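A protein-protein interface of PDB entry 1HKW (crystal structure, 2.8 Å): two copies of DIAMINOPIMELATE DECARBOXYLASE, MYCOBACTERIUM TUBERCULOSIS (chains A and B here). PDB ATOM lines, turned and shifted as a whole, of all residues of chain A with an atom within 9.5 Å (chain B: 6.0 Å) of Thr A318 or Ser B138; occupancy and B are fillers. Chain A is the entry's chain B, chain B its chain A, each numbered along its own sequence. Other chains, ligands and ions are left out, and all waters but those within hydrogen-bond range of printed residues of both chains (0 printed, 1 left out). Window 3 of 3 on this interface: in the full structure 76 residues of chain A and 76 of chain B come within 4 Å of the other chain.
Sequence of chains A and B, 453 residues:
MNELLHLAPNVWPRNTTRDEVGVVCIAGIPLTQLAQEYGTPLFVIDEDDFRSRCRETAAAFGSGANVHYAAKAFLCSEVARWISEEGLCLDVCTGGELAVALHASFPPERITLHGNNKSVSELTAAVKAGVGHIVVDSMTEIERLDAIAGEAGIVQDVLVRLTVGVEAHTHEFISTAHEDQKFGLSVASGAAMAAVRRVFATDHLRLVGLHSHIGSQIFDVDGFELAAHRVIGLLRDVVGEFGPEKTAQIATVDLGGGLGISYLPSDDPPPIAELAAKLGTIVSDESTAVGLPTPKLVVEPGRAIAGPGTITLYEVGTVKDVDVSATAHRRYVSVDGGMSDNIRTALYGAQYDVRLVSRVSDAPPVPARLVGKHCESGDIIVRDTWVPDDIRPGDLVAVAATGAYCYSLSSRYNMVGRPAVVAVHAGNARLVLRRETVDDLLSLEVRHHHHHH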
ATOM      1  N   GLU A 315      -7.274 -16.189  -8.524  1.00  0.00           N
ATOM      2  CA  GLU A 315      -6.757 -16.403  -7.161  1.00  0.00           C
ATOM      3  C   GLU A 315      -6.715 -15.075  -6.395  1.00  0.00           C
ATOM      4  O   GLU A 315      -6.217 -14.093  -6.903  1.00  0.00           O
ATOM      5  CB  GLU A 315      -5.354 -17.027  -7.177  1.00  0.00           C
ATOM      6  CG  GLU A 315      -4.887 -17.548  -5.807  1.00  0.00           C
ATOM      7  CD  GLU A 315      -3.414 -17.969  -5.776  1.00  0.00           C
ATOM      8  OE1 GLU A 315      -2.831 -18.317  -6.808  1.00  0.00           O
ATOM      9  OE2 GLU A 315      -2.842 -17.948  -4.718  1.00  0.00           O
ATOM     10  N   VAL A 316      -7.241 -15.086  -5.152  1.00  0.00           N
ATOM     11  CA  VAL A 316      -7.043 -13.989  -4.212  1.00  0.00           C
ATOM     12  C   VAL A 316      -5.583 -13.860  -3.799  1.00  0.00           C
ATOM     13  O   VAL A 316      -4.896 -14.867  -3.458  1.00  0.00           O
ATOM     14  CB  VAL A 316      -7.871 -14.152  -2.976  1.00  0.00           C
ATOM     15  CG1 VAL A 316      -7.707 -12.965  -2.079  1.00  0.00           C
ATOM     16  CG2 VAL A 316      -9.354 -14.324  -3.332  1.00  0.00           C
ATOM     17  N   GLY A 317      -5.113 -12.616  -3.837  1.00  0.00           N
ATOM     18  CA  GLY A 317      -3.774 -12.271  -3.455  1.00  0.00           C
ATOM     19  C   GLY A 317      -3.692 -11.348  -2.237  1.00  0.00           C
ATOM     20  O   GLY A 317      -2.790 -11.499  -1.410  1.00  0.00           O
ATOM     21  N   THR A 318      -4.598 -10.365  -2.152  1.00  0.00           N
ATOM     22  CA  THR A 318      -4.549  -9.404  -1.079  1.00  0.00           C
ATOM     23  C   THR A 318      -5.930  -9.103  -0.590  1.00  0.00           C
ATOM     24  O   THR A 318      -6.835  -8.969  -1.349  1.00  0.00           O
ATOM     25  CB  THR A 318      -3.820  -8.143  -1.531  1.00  0.00           C
ATOM     26  OG1 THR A 318      -2.513  -8.481  -2.014  1.00  0.00           O
ATOM     27  CG2 THR A 318      -3.519  -7.228  -0.370  1.00  0.00           C
ATOM     28  N   VAL A 319      -6.081  -9.059   0.725  1.00  0.00           N
ATOM     29  CA  VAL A 319      -7.317  -8.586   1.304  1.00  0.00           C
ATOM     30  C   VAL A 319      -7.005  -7.424   2.181  1.00  0.00           C
ATOM     31  O   VAL A 319      -6.106  -7.501   2.929  1.00  0.00           O
ATOM     32  CB  VAL A 319      -8.013  -9.629   2.103  1.00  0.00           C
ATOM     33  CG1 VAL A 319      -9.157  -9.016   2.798  1.00  0.00           C
ATOM     34  CG2 VAL A 319      -8.525 -10.711   1.225  1.00  0.00           C
ATOM     35  N   LYS A 320      -7.773  -6.328   2.025  1.00  0.00           N
ATOM     36  CA  LYS A 320      -7.544  -5.015   2.706  1.00  0.00           C
ATOM     37  C   LYS A 320      -8.855  -4.466   3.106  1.00  0.00           C
ATOM     38  O   LYS A 320      -9.706  -4.273   2.283  1.00  0.00           O
ATOM     39  CB  LYS A 320      -6.898  -4.008   1.769  1.00  0.00           C
ATOM     40  CG  LYS A 320      -6.067  -2.980   2.429  1.00  0.00           C
ATOM     41  CD  LYS A 320      -5.746  -1.812   1.476  1.00  0.00           C
ATOM     42  CE  LYS A 320      -4.271  -1.781   1.052  1.00  0.00           C
ATOM     43  NZ  LYS A 320      -3.875  -0.569   0.290  1.00  0.00           N
ATOM     44  N   ASP A 321      -9.034  -4.225   4.383  1.00  0.00           N
ATOM     45  CA  ASP A 321     -10.197  -3.524   4.872  1.00  0.00           C
ATOM     46  C   ASP A 321      -9.974  -2.010   4.686  1.00  0.00           C
ATOM     47  O   ASP A 321      -8.964  -1.481   5.077  1.00  0.00           O
ATOM     48  CB  ASP A 321     -10.409  -3.877   6.332  1.00  0.00           C
ATOM     49  CG  ASP A 321     -11.841  -4.150   6.659  1.00  0.00           C
ATOM     50  OD1 ASP A 321     -12.285  -3.616   7.733  1.00  0.00           O
ATOM     51  OD2 ASP A 321     -12.613  -4.885   5.927  1.00  0.00           O
ATOM     52  N   VAL A 322     -10.910  -1.338   4.035  1.00  0.00           N
ATOM     53  CA  VAL A 322     -10.763   0.091   3.737  1.00  0.00           C
ATOM     54  C   VAL A 322     -11.864   0.891   4.402  1.00  0.00           C
ATOM     55  O   VAL A 322     -13.004   0.611   4.216  1.00  0.00           O
ATOM     56  CB  VAL A 322     -10.746   0.365   2.213  1.00  0.00           C
ATOM     57  CG1 VAL A 322     -10.741   1.817   1.954  1.00  0.00           C
ATOM     58  CG2 VAL A 322      -9.517  -0.232   1.577  1.00  0.00           C
ATOM     59  N   ARG A 331     -14.475  -4.042   1.857  1.00  0.00           N
ATOM     60  CA  ARG A 331     -13.413  -5.059   1.831  1.00  0.00           C
ATOM     61  C   ARG A 331     -12.892  -5.169   0.416  1.00  0.00           C
ATOM     62  O   ARG A 331     -13.571  -5.677  -0.449  1.00  0.00           O
ATOM     63  CB  ARG A 331     -13.920  -6.400   2.351  1.00  0.00           C
ATOM     64  CG  ARG A 331     -12.884  -7.538   2.346  1.00  0.00           C
ATOM     65  CD  ARG A 331     -11.925  -7.608   3.548  1.00  0.00           C
ATOM     66  NE  ARG A 331     -12.620  -7.297   4.786  1.00  0.00           N
ATOM     67  CZ  ARG A 331     -13.129  -8.191   5.648  1.00  0.00           C
ATOM     68  NH1 ARG A 331     -13.773  -7.747   6.694  1.00  0.00           N
ATOM     69  NH2 ARG A 331     -12.975  -9.495   5.476  1.00  0.00           N
ATOM     70  N   TYR A 332     -11.684  -4.631   0.190  1.00  0.00           N
ATOM     71  CA  TYR A 332     -11.007  -4.711  -1.098  1.00  0.00           C
ATOM     72  C   TYR A 332     -10.230  -6.065  -1.286  1.00  0.00           C
ATOM     73  O   TYR A 332      -9.106  -6.264  -0.771  1.00  0.00           O
ATOM     74  CB  TYR A 332     -10.070  -3.530  -1.273  1.00  0.00           C
ATOM     75  CG  TYR A 332     -10.752  -2.236  -1.688  1.00  0.00           C
ATOM     76  CD1 TYR A 332     -11.490  -1.508  -0.805  1.00  0.00           C
ATOM     77  CD2 TYR A 332     -10.627  -1.723  -2.988  1.00  0.00           C
ATOM     78  CE1 TYR A 332     -12.117  -0.295  -1.205  1.00  0.00           C
ATOM     79  CE2 TYR A 332     -11.248  -0.524  -3.364  1.00  0.00           C
ATOM     80  CZ  TYR A 332     -11.975   0.175  -2.474  1.00  0.00           C
ATOM     81  OH  TYR A 332     -12.582   1.362  -2.820  1.00  0.00           O
ATOM     82  N   VAL A 333     -10.822  -6.970  -2.048  1.00  0.00           N
ATOM     83  CA  VAL A 333     -10.110  -8.175  -2.422  1.00  0.00           C
ATOM     84  C   VAL A 333      -9.500  -8.095  -3.840  1.00  0.00           C
ATOM     85  O   VAL A 333     -10.196  -7.961  -4.819  1.00  0.00           O
ATOM     86  CB  VAL A 333     -10.960  -9.515  -2.165  1.00  0.00           C
ATOM     87  CG1 VAL A 333     -12.314  -9.198  -1.519  1.00  0.00           C
ATOM     88  CG2 VAL A 333     -11.116 -10.287  -3.359  1.00  0.00           C
ATOM     89  N   SER A 334      -8.170  -8.158  -3.894  1.00  0.00           N
ATOM     90  CA  SER A 334      -7.432  -8.077  -5.115  1.00  0.00           C
ATOM     91  C   SER A 334      -7.091  -9.441  -5.610  1.00  0.00           C
ATOM     92  O   SER A 334      -7.026 -10.374  -4.893  1.00  0.00           O
ATOM     93  CB  SER A 334      -6.117  -7.290  -4.941  1.00  0.00           C
ATOM     94  OG  SER A 334      -6.205  -6.272  -4.014  1.00  0.00           O
ATOM     95  N   VAL A 335      -6.800  -9.502  -6.878  1.00  0.00           N
ATOM     96  CA  VAL A 335      -6.942 -10.698  -7.614  1.00  0.00           C
ATOM     97  C   VAL A 335      -5.882 -10.699  -8.717  1.00  0.00           C
ATOM     98  O   VAL A 335      -5.289  -9.718  -9.013  1.00  0.00           O
ATOM     99  CB  VAL A 335      -8.398 -10.769  -8.112  1.00  0.00           C
ATOM    100  CG1 VAL A 335      -8.483 -10.941  -9.493  1.00  0.00           C
ATOM    101  CG2 VAL A 335      -9.141 -11.848  -7.401  1.00  0.00           C
ATOM    102  N   ASP A 336      -5.610 -11.864  -9.228  1.00  0.00           N
ATOM    103  CA  ASP A 336      -4.579 -12.217 -10.235  1.00  0.00           C
ATOM    104  C   ASP A 336      -4.603 -11.293 -11.514  1.00  0.00           C
ATOM    105  O   ASP A 336      -3.588 -11.166 -12.207  1.00  0.00           O
ATOM    106  CB  ASP A 336      -4.983 -13.591 -10.695  1.00  0.00           C
ATOM    107  CG  ASP A 336      -3.981 -14.526 -10.547  1.00  0.00           C
ATOM    108  OD1 ASP A 336      -2.815 -14.418 -11.221  1.00  0.00           O
ATOM    109  OD2 ASP A 336      -4.212 -15.515  -9.901  1.00  0.00           O
ATOM    110  N   ARG A 369     -15.250  -5.011  -2.785  1.00  0.00           N
ATOM    111  CA  ARG A 369     -14.847  -4.564  -4.122  1.00  0.00           C
ATOM    112  C   ARG A 369     -13.786  -5.510  -4.623  1.00  0.00           C
ATOM    113  O   ARG A 369     -12.785  -5.719  -3.974  1.00  0.00           O
ATOM    114  CB  ARG A 369     -14.277  -3.105  -4.110  1.00  0.00           C
ATOM    115  CG  ARG A 369     -15.046  -2.114  -4.991  1.00  0.00           C
ATOM    116  CD  ARG A 369     -14.257  -0.974  -5.559  1.00  0.00           C
ATOM    117  NE  ARG A 369     -14.674   0.414  -5.114  1.00  0.00           N
ATOM    118  CZ  ARG A 369     -15.935   0.847  -4.873  1.00  0.00           C
ATOM    119  NH1 ARG A 369     -16.974   0.055  -4.951  1.00  0.00           N
ATOM    120  NH2 ARG A 369     -16.141   2.103  -4.499  1.00  0.00           N
ATOM    121  N   LEU A 370     -14.015  -6.073  -5.787  1.00  0.00           N
ATOM    122  CA  LEU A 370     -13.106  -6.979  -6.369  1.00  0.00           C
ATOM    123  C   LEU A 370     -12.318  -6.205  -7.303  1.00  0.00           C
ATOM    124  O   LEU A 370     -12.846  -5.433  -8.106  1.00  0.00           O
ATOM    125  CB  LEU A 370     -13.863  -8.069  -7.115  1.00  0.00           C
ATOM    126  CG  LEU A 370     -12.980  -9.273  -7.571  1.00  0.00           C
ATOM    127  CD1 LEU A 370     -12.591 -10.178  -6.392  1.00  0.00           C
ATOM    128  CD2 LEU A 370     -13.680 -10.094  -8.661  1.00  0.00           C
ATOM    129  N   VAL A 371     -11.045  -6.393  -7.253  1.00  0.00           N
ATOM    130  CA  VAL A 371     -10.178  -5.378  -7.731  1.00  0.00           C
ATOM    131  C   VAL A 371      -8.982  -6.017  -8.398  1.00  0.00           C
ATOM    132  O   VAL A 371      -8.516  -7.079  -7.970  1.00  0.00           O
ATOM    133  CB  VAL A 371      -9.800  -4.531  -6.548  1.00  0.00           C
ATOM    134  CG1 VAL A 371      -8.283  -4.535  -6.298  1.00  0.00           C
ATOM    135  CG2 VAL A 371     -10.383  -3.154  -6.684  1.00  0.00           C
ATOM    136  N   GLY A 372      -8.490  -5.423  -9.465  1.00  0.00           N
ATOM    137  CA  GLY A 372      -7.361  -6.031 -10.186  1.00  0.00           C
ATOM    138  C   GLY A 372      -5.993  -5.648  -9.643  1.00  0.00           C
ATOM    139  O   GLY A 372      -5.877  -4.974  -8.611  1.00  0.00           O
ATOM    140  N   LYS A 373      -4.956  -6.026 -10.350  1.00  0.00           N
ATOM    141  CA  LYS A 373      -3.613  -5.788  -9.860  1.00  0.00           C
ATOM    142  C   LYS A 373      -2.865  -4.719 -10.618  1.00  0.00           C
ATOM    143  O   LYS A 373      -1.704  -4.532 -10.367  1.00  0.00           O
ATOM    144  CB  LYS A 373      -2.810  -7.062  -9.893  1.00  0.00           C
ATOM    145  CG  LYS A 373      -2.176  -7.336 -11.218  1.00  0.00           C
ATOM    146  CD  LYS A 373      -1.965  -8.789 -11.396  1.00  0.00           C
ATOM    147  CE  LYS A 373      -0.503  -9.198 -11.262  1.00  0.00           C
ATOM    148  NZ  LYS A 373      -0.391 -10.532 -11.805  1.00  0.00           N
ATOM    149  N   VAL A 387     -18.739 -10.442   0.026  1.00  0.00           N
ATOM    150  CA  VAL A 387     -17.746 -11.441   0.120  1.00  0.00           C
ATOM    151  C   VAL A 387     -17.820 -12.004   1.552  1.00  0.00           C
ATOM    152  O   VAL A 387     -18.239 -11.317   2.485  1.00  0.00           O
ATOM    153  CB  VAL A 387     -16.445 -10.801  -0.178  1.00  0.00           C
ATOM    154  CG1 VAL A 387     -15.458 -11.182   0.773  1.00  0.00           C
ATOM    155  CG2 VAL A 387     -16.018 -11.135  -1.579  1.00  0.00           C
ATOM    156  N   ILE A 391     -12.667 -14.529   3.854  1.00  0.00           N
ATOM    157  CA  ILE A 391     -11.956 -14.537   2.600  1.00  0.00           C
ATOM    158  C   ILE A 391     -10.532 -14.111   2.768  1.00  0.00           C
ATOM    159  O   ILE A 391     -10.221 -13.193   3.511  1.00  0.00           O
ATOM    160  CB  ILE A 391     -12.643 -13.623   1.569  1.00  0.00           C
ATOM    161  CG1 ILE A 391     -12.299 -14.112   0.167  1.00  0.00           C
ATOM    162  CG2 ILE A 391     -12.201 -12.211   1.734  1.00  0.00           C
ATOM    163  CD1 ILE A 391     -12.988 -13.428  -0.892  1.00  0.00           C
ATOM    164  N   ARG A 392      -9.669 -14.744   2.029  1.00  0.00           N
ATOM    165  CA  ARG A 392      -8.302 -14.829   2.424  1.00  0.00           C
ATOM    166  C   ARG A 392      -7.465 -15.260   1.247  1.00  0.00           C
ATOM    167  O   ARG A 392      -7.898 -16.073   0.442  1.00  0.00           O
ATOM    168  CB  ARG A 392      -8.213 -15.847   3.583  1.00  0.00           C
ATOM    169  CG  ARG A 392      -7.024 -16.860   3.569  1.00  0.00           C
ATOM    170  CD  ARG A 392      -7.458 -18.412   3.637  1.00  0.00           C
ATOM    171  NE  ARG A 392      -8.426 -18.716   4.700  1.00  0.00           N
ATOM    172  CZ  ARG A 392      -9.047 -19.914   4.839  1.00  0.00           C
ATOM    173  NH1 ARG A 392      -9.924 -20.095   5.838  1.00  0.00           N
ATOM    174  NH2 ARG A 392      -8.800 -20.945   3.966  1.00  0.00           N
ATOM    175  N   PRO A 393      -6.254 -14.739   1.141  1.00  0.00           N
ATOM    176  CA  PRO A 393      -5.397 -15.069  -0.016  1.00  0.00           C
ATOM    177  C   PRO A 393      -5.143 -16.537  -0.118  1.00  0.00           C
ATOM    178  O   PRO A 393      -4.965 -17.178   0.891  1.00  0.00           O
ATOM    179  CB  PRO A 393      -4.091 -14.297   0.239  1.00  0.00           C
ATOM    180  CG  PRO A 393      -4.189 -13.693   1.570  1.00  0.00           C
ATOM    181  CD  PRO A 393      -5.619 -13.803   2.078  1.00  0.00           C
ATOM    182  N   GLY A 394      -5.153 -17.058  -1.347  1.00  0.00           N
ATOM    183  CA  GLY A 394      -5.243 -18.477  -1.594  1.00  0.00           C
ATOM    184  C   GLY A 394      -6.615 -18.901  -2.101  1.00  0.00           C
ATOM    185  O   GLY A 394      -6.745 -19.883  -2.799  1.00  0.00           O
ATOM    186  N   ASP A 395      -7.657 -18.184  -1.723  1.00  0.00           N
ATOM    187  CA  ASP A 395      -9.023 -18.613  -2.062  1.00  0.00           C
ATOM    188  C   ASP A 395      -9.204 -18.350  -3.541  1.00  0.00           C
ATOM    189  O   ASP A 395      -8.557 -17.467  -4.089  1.00  0.00           O
ATOM    190  CB  ASP A 395     -10.082 -17.819  -1.259  1.00  0.00           C
ATOM    191  CG  ASP A 395     -10.302 -18.344   0.178  1.00  0.00           C
ATOM    192  OD1 ASP A 395      -9.933 -19.509   0.512  1.00  0.00           O
ATOM    193  OD2 ASP A 395     -10.857 -17.630   1.036  1.00  0.00           O
ATOM    194  N   ASN B 116      -0.693  -2.939  -6.177  1.00  0.00           N
ATOM    195  CA  ASN B 116      -1.595  -3.292  -5.104  1.00  0.00           C
ATOM    196  C   ASN B 116      -1.671  -4.776  -4.733  1.00  0.00           C
ATOM    197  O   ASN B 116      -2.222  -5.110  -3.678  1.00  0.00           O
ATOM    198  CB  ASN B 116      -3.001  -2.759  -5.370  1.00  0.00           C
ATOM    199  CG  ASN B 116      -3.700  -3.491  -6.444  1.00  0.00           C
ATOM    200  OD1 ASN B 116      -3.402  -3.291  -7.633  1.00  0.00           O
ATOM    201  ND2 ASN B 116      -4.672  -4.341  -6.064  1.00  0.00           N
ATOM    202  N   ASN B 117      -1.122  -5.646  -5.563  1.00  0.00           N
ATOM    203  CA  ASN B 117      -1.266  -7.093  -5.361  1.00  0.00           C
ATOM    204  C   ASN B 117      -0.078  -7.813  -5.836  1.00  0.00           C
ATOM    205  O   ASN B 117      -0.198  -8.707  -6.633  1.00  0.00           O
ATOM    206  CB  ASN B 117      -2.502  -7.606  -6.105  1.00  0.00           C
ATOM    207  CG  ASN B 117      -2.835  -9.089  -5.794  1.00  0.00           C
ATOM    208  OD1 ASN B 117      -2.532  -9.598  -4.718  1.00  0.00           O
ATOM    209  ND2 ASN B 117      -3.468  -9.771  -6.754  1.00  0.00           N
ATOM    210  N   LYS B 118       1.099  -7.415  -5.360  1.00  0.00           N
ATOM    211  CA  LYS B 118       2.325  -8.121  -5.755  1.00  0.00           C
ATOM    212  C   LYS B 118       2.256  -9.664  -5.387  1.00  0.00           C
ATOM    213  O   LYS B 118       1.865 -10.025  -4.286  1.00  0.00           O
ATOM    214  CB  LYS B 118       3.527  -7.493  -5.099  1.00  0.00           C
ATOM    215  CG  LYS B 118       4.215  -6.379  -5.877  1.00  0.00           C
ATOM    216  CD  LYS B 118       3.808  -5.051  -5.338  1.00  0.00           C
ATOM    217  CE  LYS B 118       4.943  -4.125  -4.988  1.00  0.00           C
ATOM    218  NZ  LYS B 118       4.330  -2.918  -4.320  1.00  0.00           N
ATOM    219  N   VAL B 136       5.609  -0.555  -0.820  1.00  0.00           N
ATOM    220  CA  VAL B 136       4.688  -1.524  -0.274  1.00  0.00           C
ATOM    221  C   VAL B 136       3.279  -0.958  -0.048  1.00  0.00           C
ATOM    222  O   VAL B 136       3.101   0.228   0.244  1.00  0.00           O
ATOM    223  CB  VAL B 136       5.236  -2.106   1.045  1.00  0.00           C
ATOM    224  CG1 VAL B 136       6.582  -2.789   0.803  1.00  0.00           C
ATOM    225  CG2 VAL B 136       5.324  -0.994   2.184  1.00  0.00           C
ATOM    226  N   ASP B 137       2.288  -1.816  -0.146  1.00  0.00           N
ATOM    227  CA  ASP B 137       0.931  -1.358  -0.282  1.00  0.00           C
ATOM    228  C   ASP B 137      -0.066  -1.996   0.683  1.00  0.00           C
ATOM    229  O   ASP B 137      -1.106  -1.439   0.939  1.00  0.00           O
ATOM    230  CB  ASP B 137       0.471  -1.633  -1.697  1.00  0.00           C
ATOM    231  CG  ASP B 137      -0.818  -0.904  -2.045  1.00  0.00           C
ATOM    232  OD1 ASP B 137      -0.695   0.325  -2.296  1.00  0.00           O
ATOM    233  OD2 ASP B 137      -1.994  -1.483  -2.067  1.00  0.00           O
ATOM    234  N   SER B 138       0.237  -3.179   1.156  1.00  0.00           N
ATOM    235  CA  SER B 138      -0.519  -3.794   2.213  1.00  0.00           C
ATOM    236  C   SER B 138       0.379  -4.272   3.367  1.00  0.00           C
ATOM    237  O   SER B 138       1.559  -4.272   3.271  1.00  0.00           O
ATOM    238  CB  SER B 138      -1.326  -4.961   1.672  1.00  0.00           C
ATOM    239  OG  SER B 138      -0.515  -5.840   0.971  1.00  0.00           O
ATOM    240  N   MET B 139      -0.254  -4.644   4.468  1.00  0.00           N
ATOM    241  CA  MET B 139       0.403  -5.323   5.552  1.00  0.00           C
ATOM    242  C   MET B 139       0.819  -6.713   5.126  1.00  0.00           C
ATOM    243  O   MET B 139       1.856  -7.189   5.533  1.00  0.00           O
ATOM    244  CB  MET B 139      -0.519  -5.408   6.751  1.00  0.00           C
ATOM    245  CG  MET B 139      -0.874  -4.093   7.334  1.00  0.00           C
ATOM    246  SD  MET B 139       0.647  -3.097   8.112  1.00  0.00           S
ATOM    247  CE  MET B 139       1.006  -4.333   9.753  1.00  0.00           C
ATOM    248  N   THR B 140       0.013  -7.370   4.309  1.00  0.00           N
ATOM    249  CA  THR B 140       0.404  -8.670   3.768  1.00  0.00           C
ATOM    250  C   THR B 140       1.680  -8.592   2.922  1.00  0.00           C
ATOM    251  O   THR B 140       2.484  -9.457   2.969  1.00  0.00           O
ATOM    252  CB  THR B 140      -0.720  -9.266   2.890  1.00  0.00           C
ATOM    253  OG1 THR B 140      -1.931  -9.273   3.605  1.00  0.00           O
ATOM    254  CG2 THR B 140      -0.475 -10.758   2.606  1.00  0.00           C
ATOM    255  N   GLU B 141       1.818  -7.555   2.125  1.00  0.00           N
ATOM    256  CA  GLU B 141       2.974  -7.425   1.274  1.00  0.00           C
ATOM    257  C   GLU B 141       4.195  -7.371   2.147  1.00  0.00           C
ATOM    258  O   GLU B 141       5.252  -7.935   1.807  1.00  0.00           O
ATOM    259  CB  GLU B 141       2.892  -6.156   0.422  1.00  0.00           C
ATOM    260  CG  GLU B 141       3.770  -6.200  -0.813  1.00  0.00           C
ATOM    261  CD  GLU B 141       3.771  -4.909  -1.607  1.00  0.00           C
ATOM    262  OE1 GLU B 141       2.702  -4.468  -2.096  1.00  0.00           O
ATOM    263  OE2 GLU B 141       4.836  -4.360  -1.782  1.00  0.00           O
ATOM    264  N   ILE B 142       4.061  -6.699   3.279  1.00  0.00           N
ATOM    265  CA  ILE B 142       5.176  -6.500   4.142  1.00  0.00           C
ATOM    266  C   ILE B 142       5.611  -7.835   4.746  1.00  0.00           C
ATOM    267  O   ILE B 142       6.798  -8.181   4.684  1.00  0.00           O
ATOM    268  CB  ILE B 142       4.866  -5.480   5.219  1.00  0.00           C
ATOM    269  CG1 ILE B 142       4.718  -4.086   4.615  1.00  0.00           C
ATOM    270  CG2 ILE B 142       5.979  -5.436   6.204  1.00  0.00           C
ATOM    271  CD1 ILE B 142       4.142  -3.091   5.540  1.00  0.00           C
ATOM    272  N   GLU B 143       4.673  -8.609   5.295  1.00  0.00           N
ATOM    273  CA  GLU B 143       5.049  -9.899   5.841  1.00  0.00           C
ATOM    274  C   GLU B 143       5.762 -10.697   4.720  1.00  0.00           C
ATOM    275  O   GLU B 143       6.840 -11.332   4.930  1.00  0.00           O
ATOM    276  CB  GLU B 143       3.862 -10.694   6.429  1.00  0.00           C
ATOM    277  CG  GLU B 143       2.825  -9.937   7.359  1.00  0.00           C
ATOM    278  CD  GLU B 143       3.383  -9.373   8.761  1.00  0.00           C
ATOM    279  OE1 GLU B 143       2.680  -8.415   9.354  1.00  0.00           O
ATOM    280  OE2 GLU B 143       4.481  -9.874   9.288  1.00  0.00           O
ATOM    281  N   ARG B 144       5.210 -10.621   3.527  1.00  0.00           N
ATOM    282  CA  ARG B 144       5.718 -11.388   2.395  1.00  0.00           C
ATOM    283  C   ARG B 144       7.159 -10.971   1.969  1.00  0.00           C
ATOM    284  O   ARG B 144       8.007 -11.812   1.721  1.00  0.00           O
ATOM    285  CB  ARG B 144       4.784 -11.224   1.209  1.00  0.00           C
ATOM    286  CG  ARG B 144       3.571 -12.089   1.226  1.00  0.00           C
ATOM    287  CD  ARG B 144       2.678 -11.857  -0.009  1.00  0.00           C
ATOM    288  NE  ARG B 144       1.481 -12.689  -0.023  1.00  0.00           N
ATOM    289  CZ  ARG B 144       0.307 -12.294  -0.436  1.00  0.00           C
ATOM    290  NH1 ARG B 144      -0.719 -13.111  -0.404  1.00  0.00           N
ATOM    291  NH2 ARG B 144       0.138 -11.064  -0.868  1.00  0.00           N
ATOM    292  N   LEU B 185      -2.233   3.039   2.475  1.00  0.00           N
ATOM    293  CA  LEU B 185      -2.667   2.845   3.818  1.00  0.00           C
ATOM    294  C   LEU B 185      -3.039   4.176   4.380  1.00  0.00           C
ATOM    295  O   LEU B 185      -2.285   5.149   4.268  1.00  0.00           O
ATOM    296  CB  LEU B 185      -1.585   2.124   4.619  1.00  0.00           C
ATOM    297  CG  LEU B 185      -1.368   0.664   4.067  1.00  0.00           C
ATOM    298  CD1 LEU B 185      -0.092   0.093   4.509  1.00  0.00           C
ATOM    299  CD2 LEU B 185      -2.475  -0.263   4.473  1.00  0.00           C
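Thr A318 touches four residues of chain B. Of chain A, only Thr A318 (3.6 Å) comes within 4 Å of Ser B138. Of chain A, only Gly A317 (3.2 Å), Thr A318 (2.9 Å), Ser A334 (3.8 Å), Val A335 (2.9 Å), Asp A336 (3.9 Å) and Lys A373 (3.8 Å) come within 4 Å of Asn B117. Asp B137 touches one residue of chain A. Thr B140 touches none of the printed residues of chain A. Of the printed residues of chain B, Gly A317 touches Asn B117 (3.2 Å) and Arg B144 (2.8 Å). Of the printed residues of chain B, Lys A320 touches Asp B137. Of the printed residues of chain A, Arg B144 touches Gly A317, Thr A318 and Pro A393. The nearest residue of chain B that does not touch Thr A318 is Thr B140 (4.7 Å). The nearest printed residue of chain B that does not touch Lys A320 is Leu B185 (4.2 Å).
Of the 25 printed residues of chain A, 10 touch a printed residue of chain B. Along chain B the printed residues that touch a printed residue of chain A span positions 116 to 144. Among the printed residues, Asp or Glu carboxylates within 4 Å of a Lys or Arg side-chain nitrogen of the other chain: Lys A320 with Asp B137 (3.2 Å).
No position is printed for both chains. Of the 16 pairs that touch across the chains among the printed residues, none has its exchanged pair printed and touching as well.
ND2 of Asn B116 sits at hydrogen-bond distance from OG of Ser A334 (3.2 Å). The backbone carbonyl oxygen (O) of Lys A373 sits close to the side-chain amide oxygen (OD1) of Asn B116 (3.4 Å). The backbone carbonyl oxygen of Gly A372 lies within hydrogen-bond range of the side-chain amide nitrogen of Asn B116 (2.9 Å). The side-chain carboxylate (OD2) of Asp B137 is in salt-bridge range of the side-chain amino group (NZ) of Lys A320, at 3.2 Å. The side-chain amide oxygen of Asn B117 sits at hydrogen-bond distance from the side-chain hydroxyl of Thr A318. ND2 of Asn B117 sits at hydrogen-bond distance from O of Val A335. The backbone carbonyl oxygen (O) of Gly A317 is in hydrogen-bond range of the guanidinium group (NH1) of Arg B144 (2.8 Å).
Among the printed residues, pairs that only touch across the chains: Gly A317 with Asn B117 (3.2 Å), Thr A318 with Ser B138 (3.6 Å), Val A371 with Asn B116 (3.6 Å), Pro A393 with Arg B144 (3.6 Å), Thr A318 with Asn B116 (3.8 Å), Ser A334 with Asn B117 (3.8 Å), Lys A373 with Asn B117 (3.8 Å), Thr A318 with Arg B144 (3.9 Å) and Asp A336 with Asn B117 (3.9 Å).
N of Asp A336 is in hydrogen-bond range of O of Glu A315 (3.3 Å). The backbone carbonyl oxygen (O) of Thr A318 sits at hydrogen-bond distance from the backbone NH (N) of Ser A334 (3.0 Å). N of Asp B137 sits at hydrogen-bond distance from OE1 of Glu B141 (3.3 Å). The backbone NH of Val A335 is in hydrogen-bond range of the backbone carbonyl oxygen of Val A371, 3.2 Å away. The side-chain hydroxyl (OG) of Ser B138 is in hydrogen-bond range of the backbone NH (N) of Glu B141 (3.1 Å).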
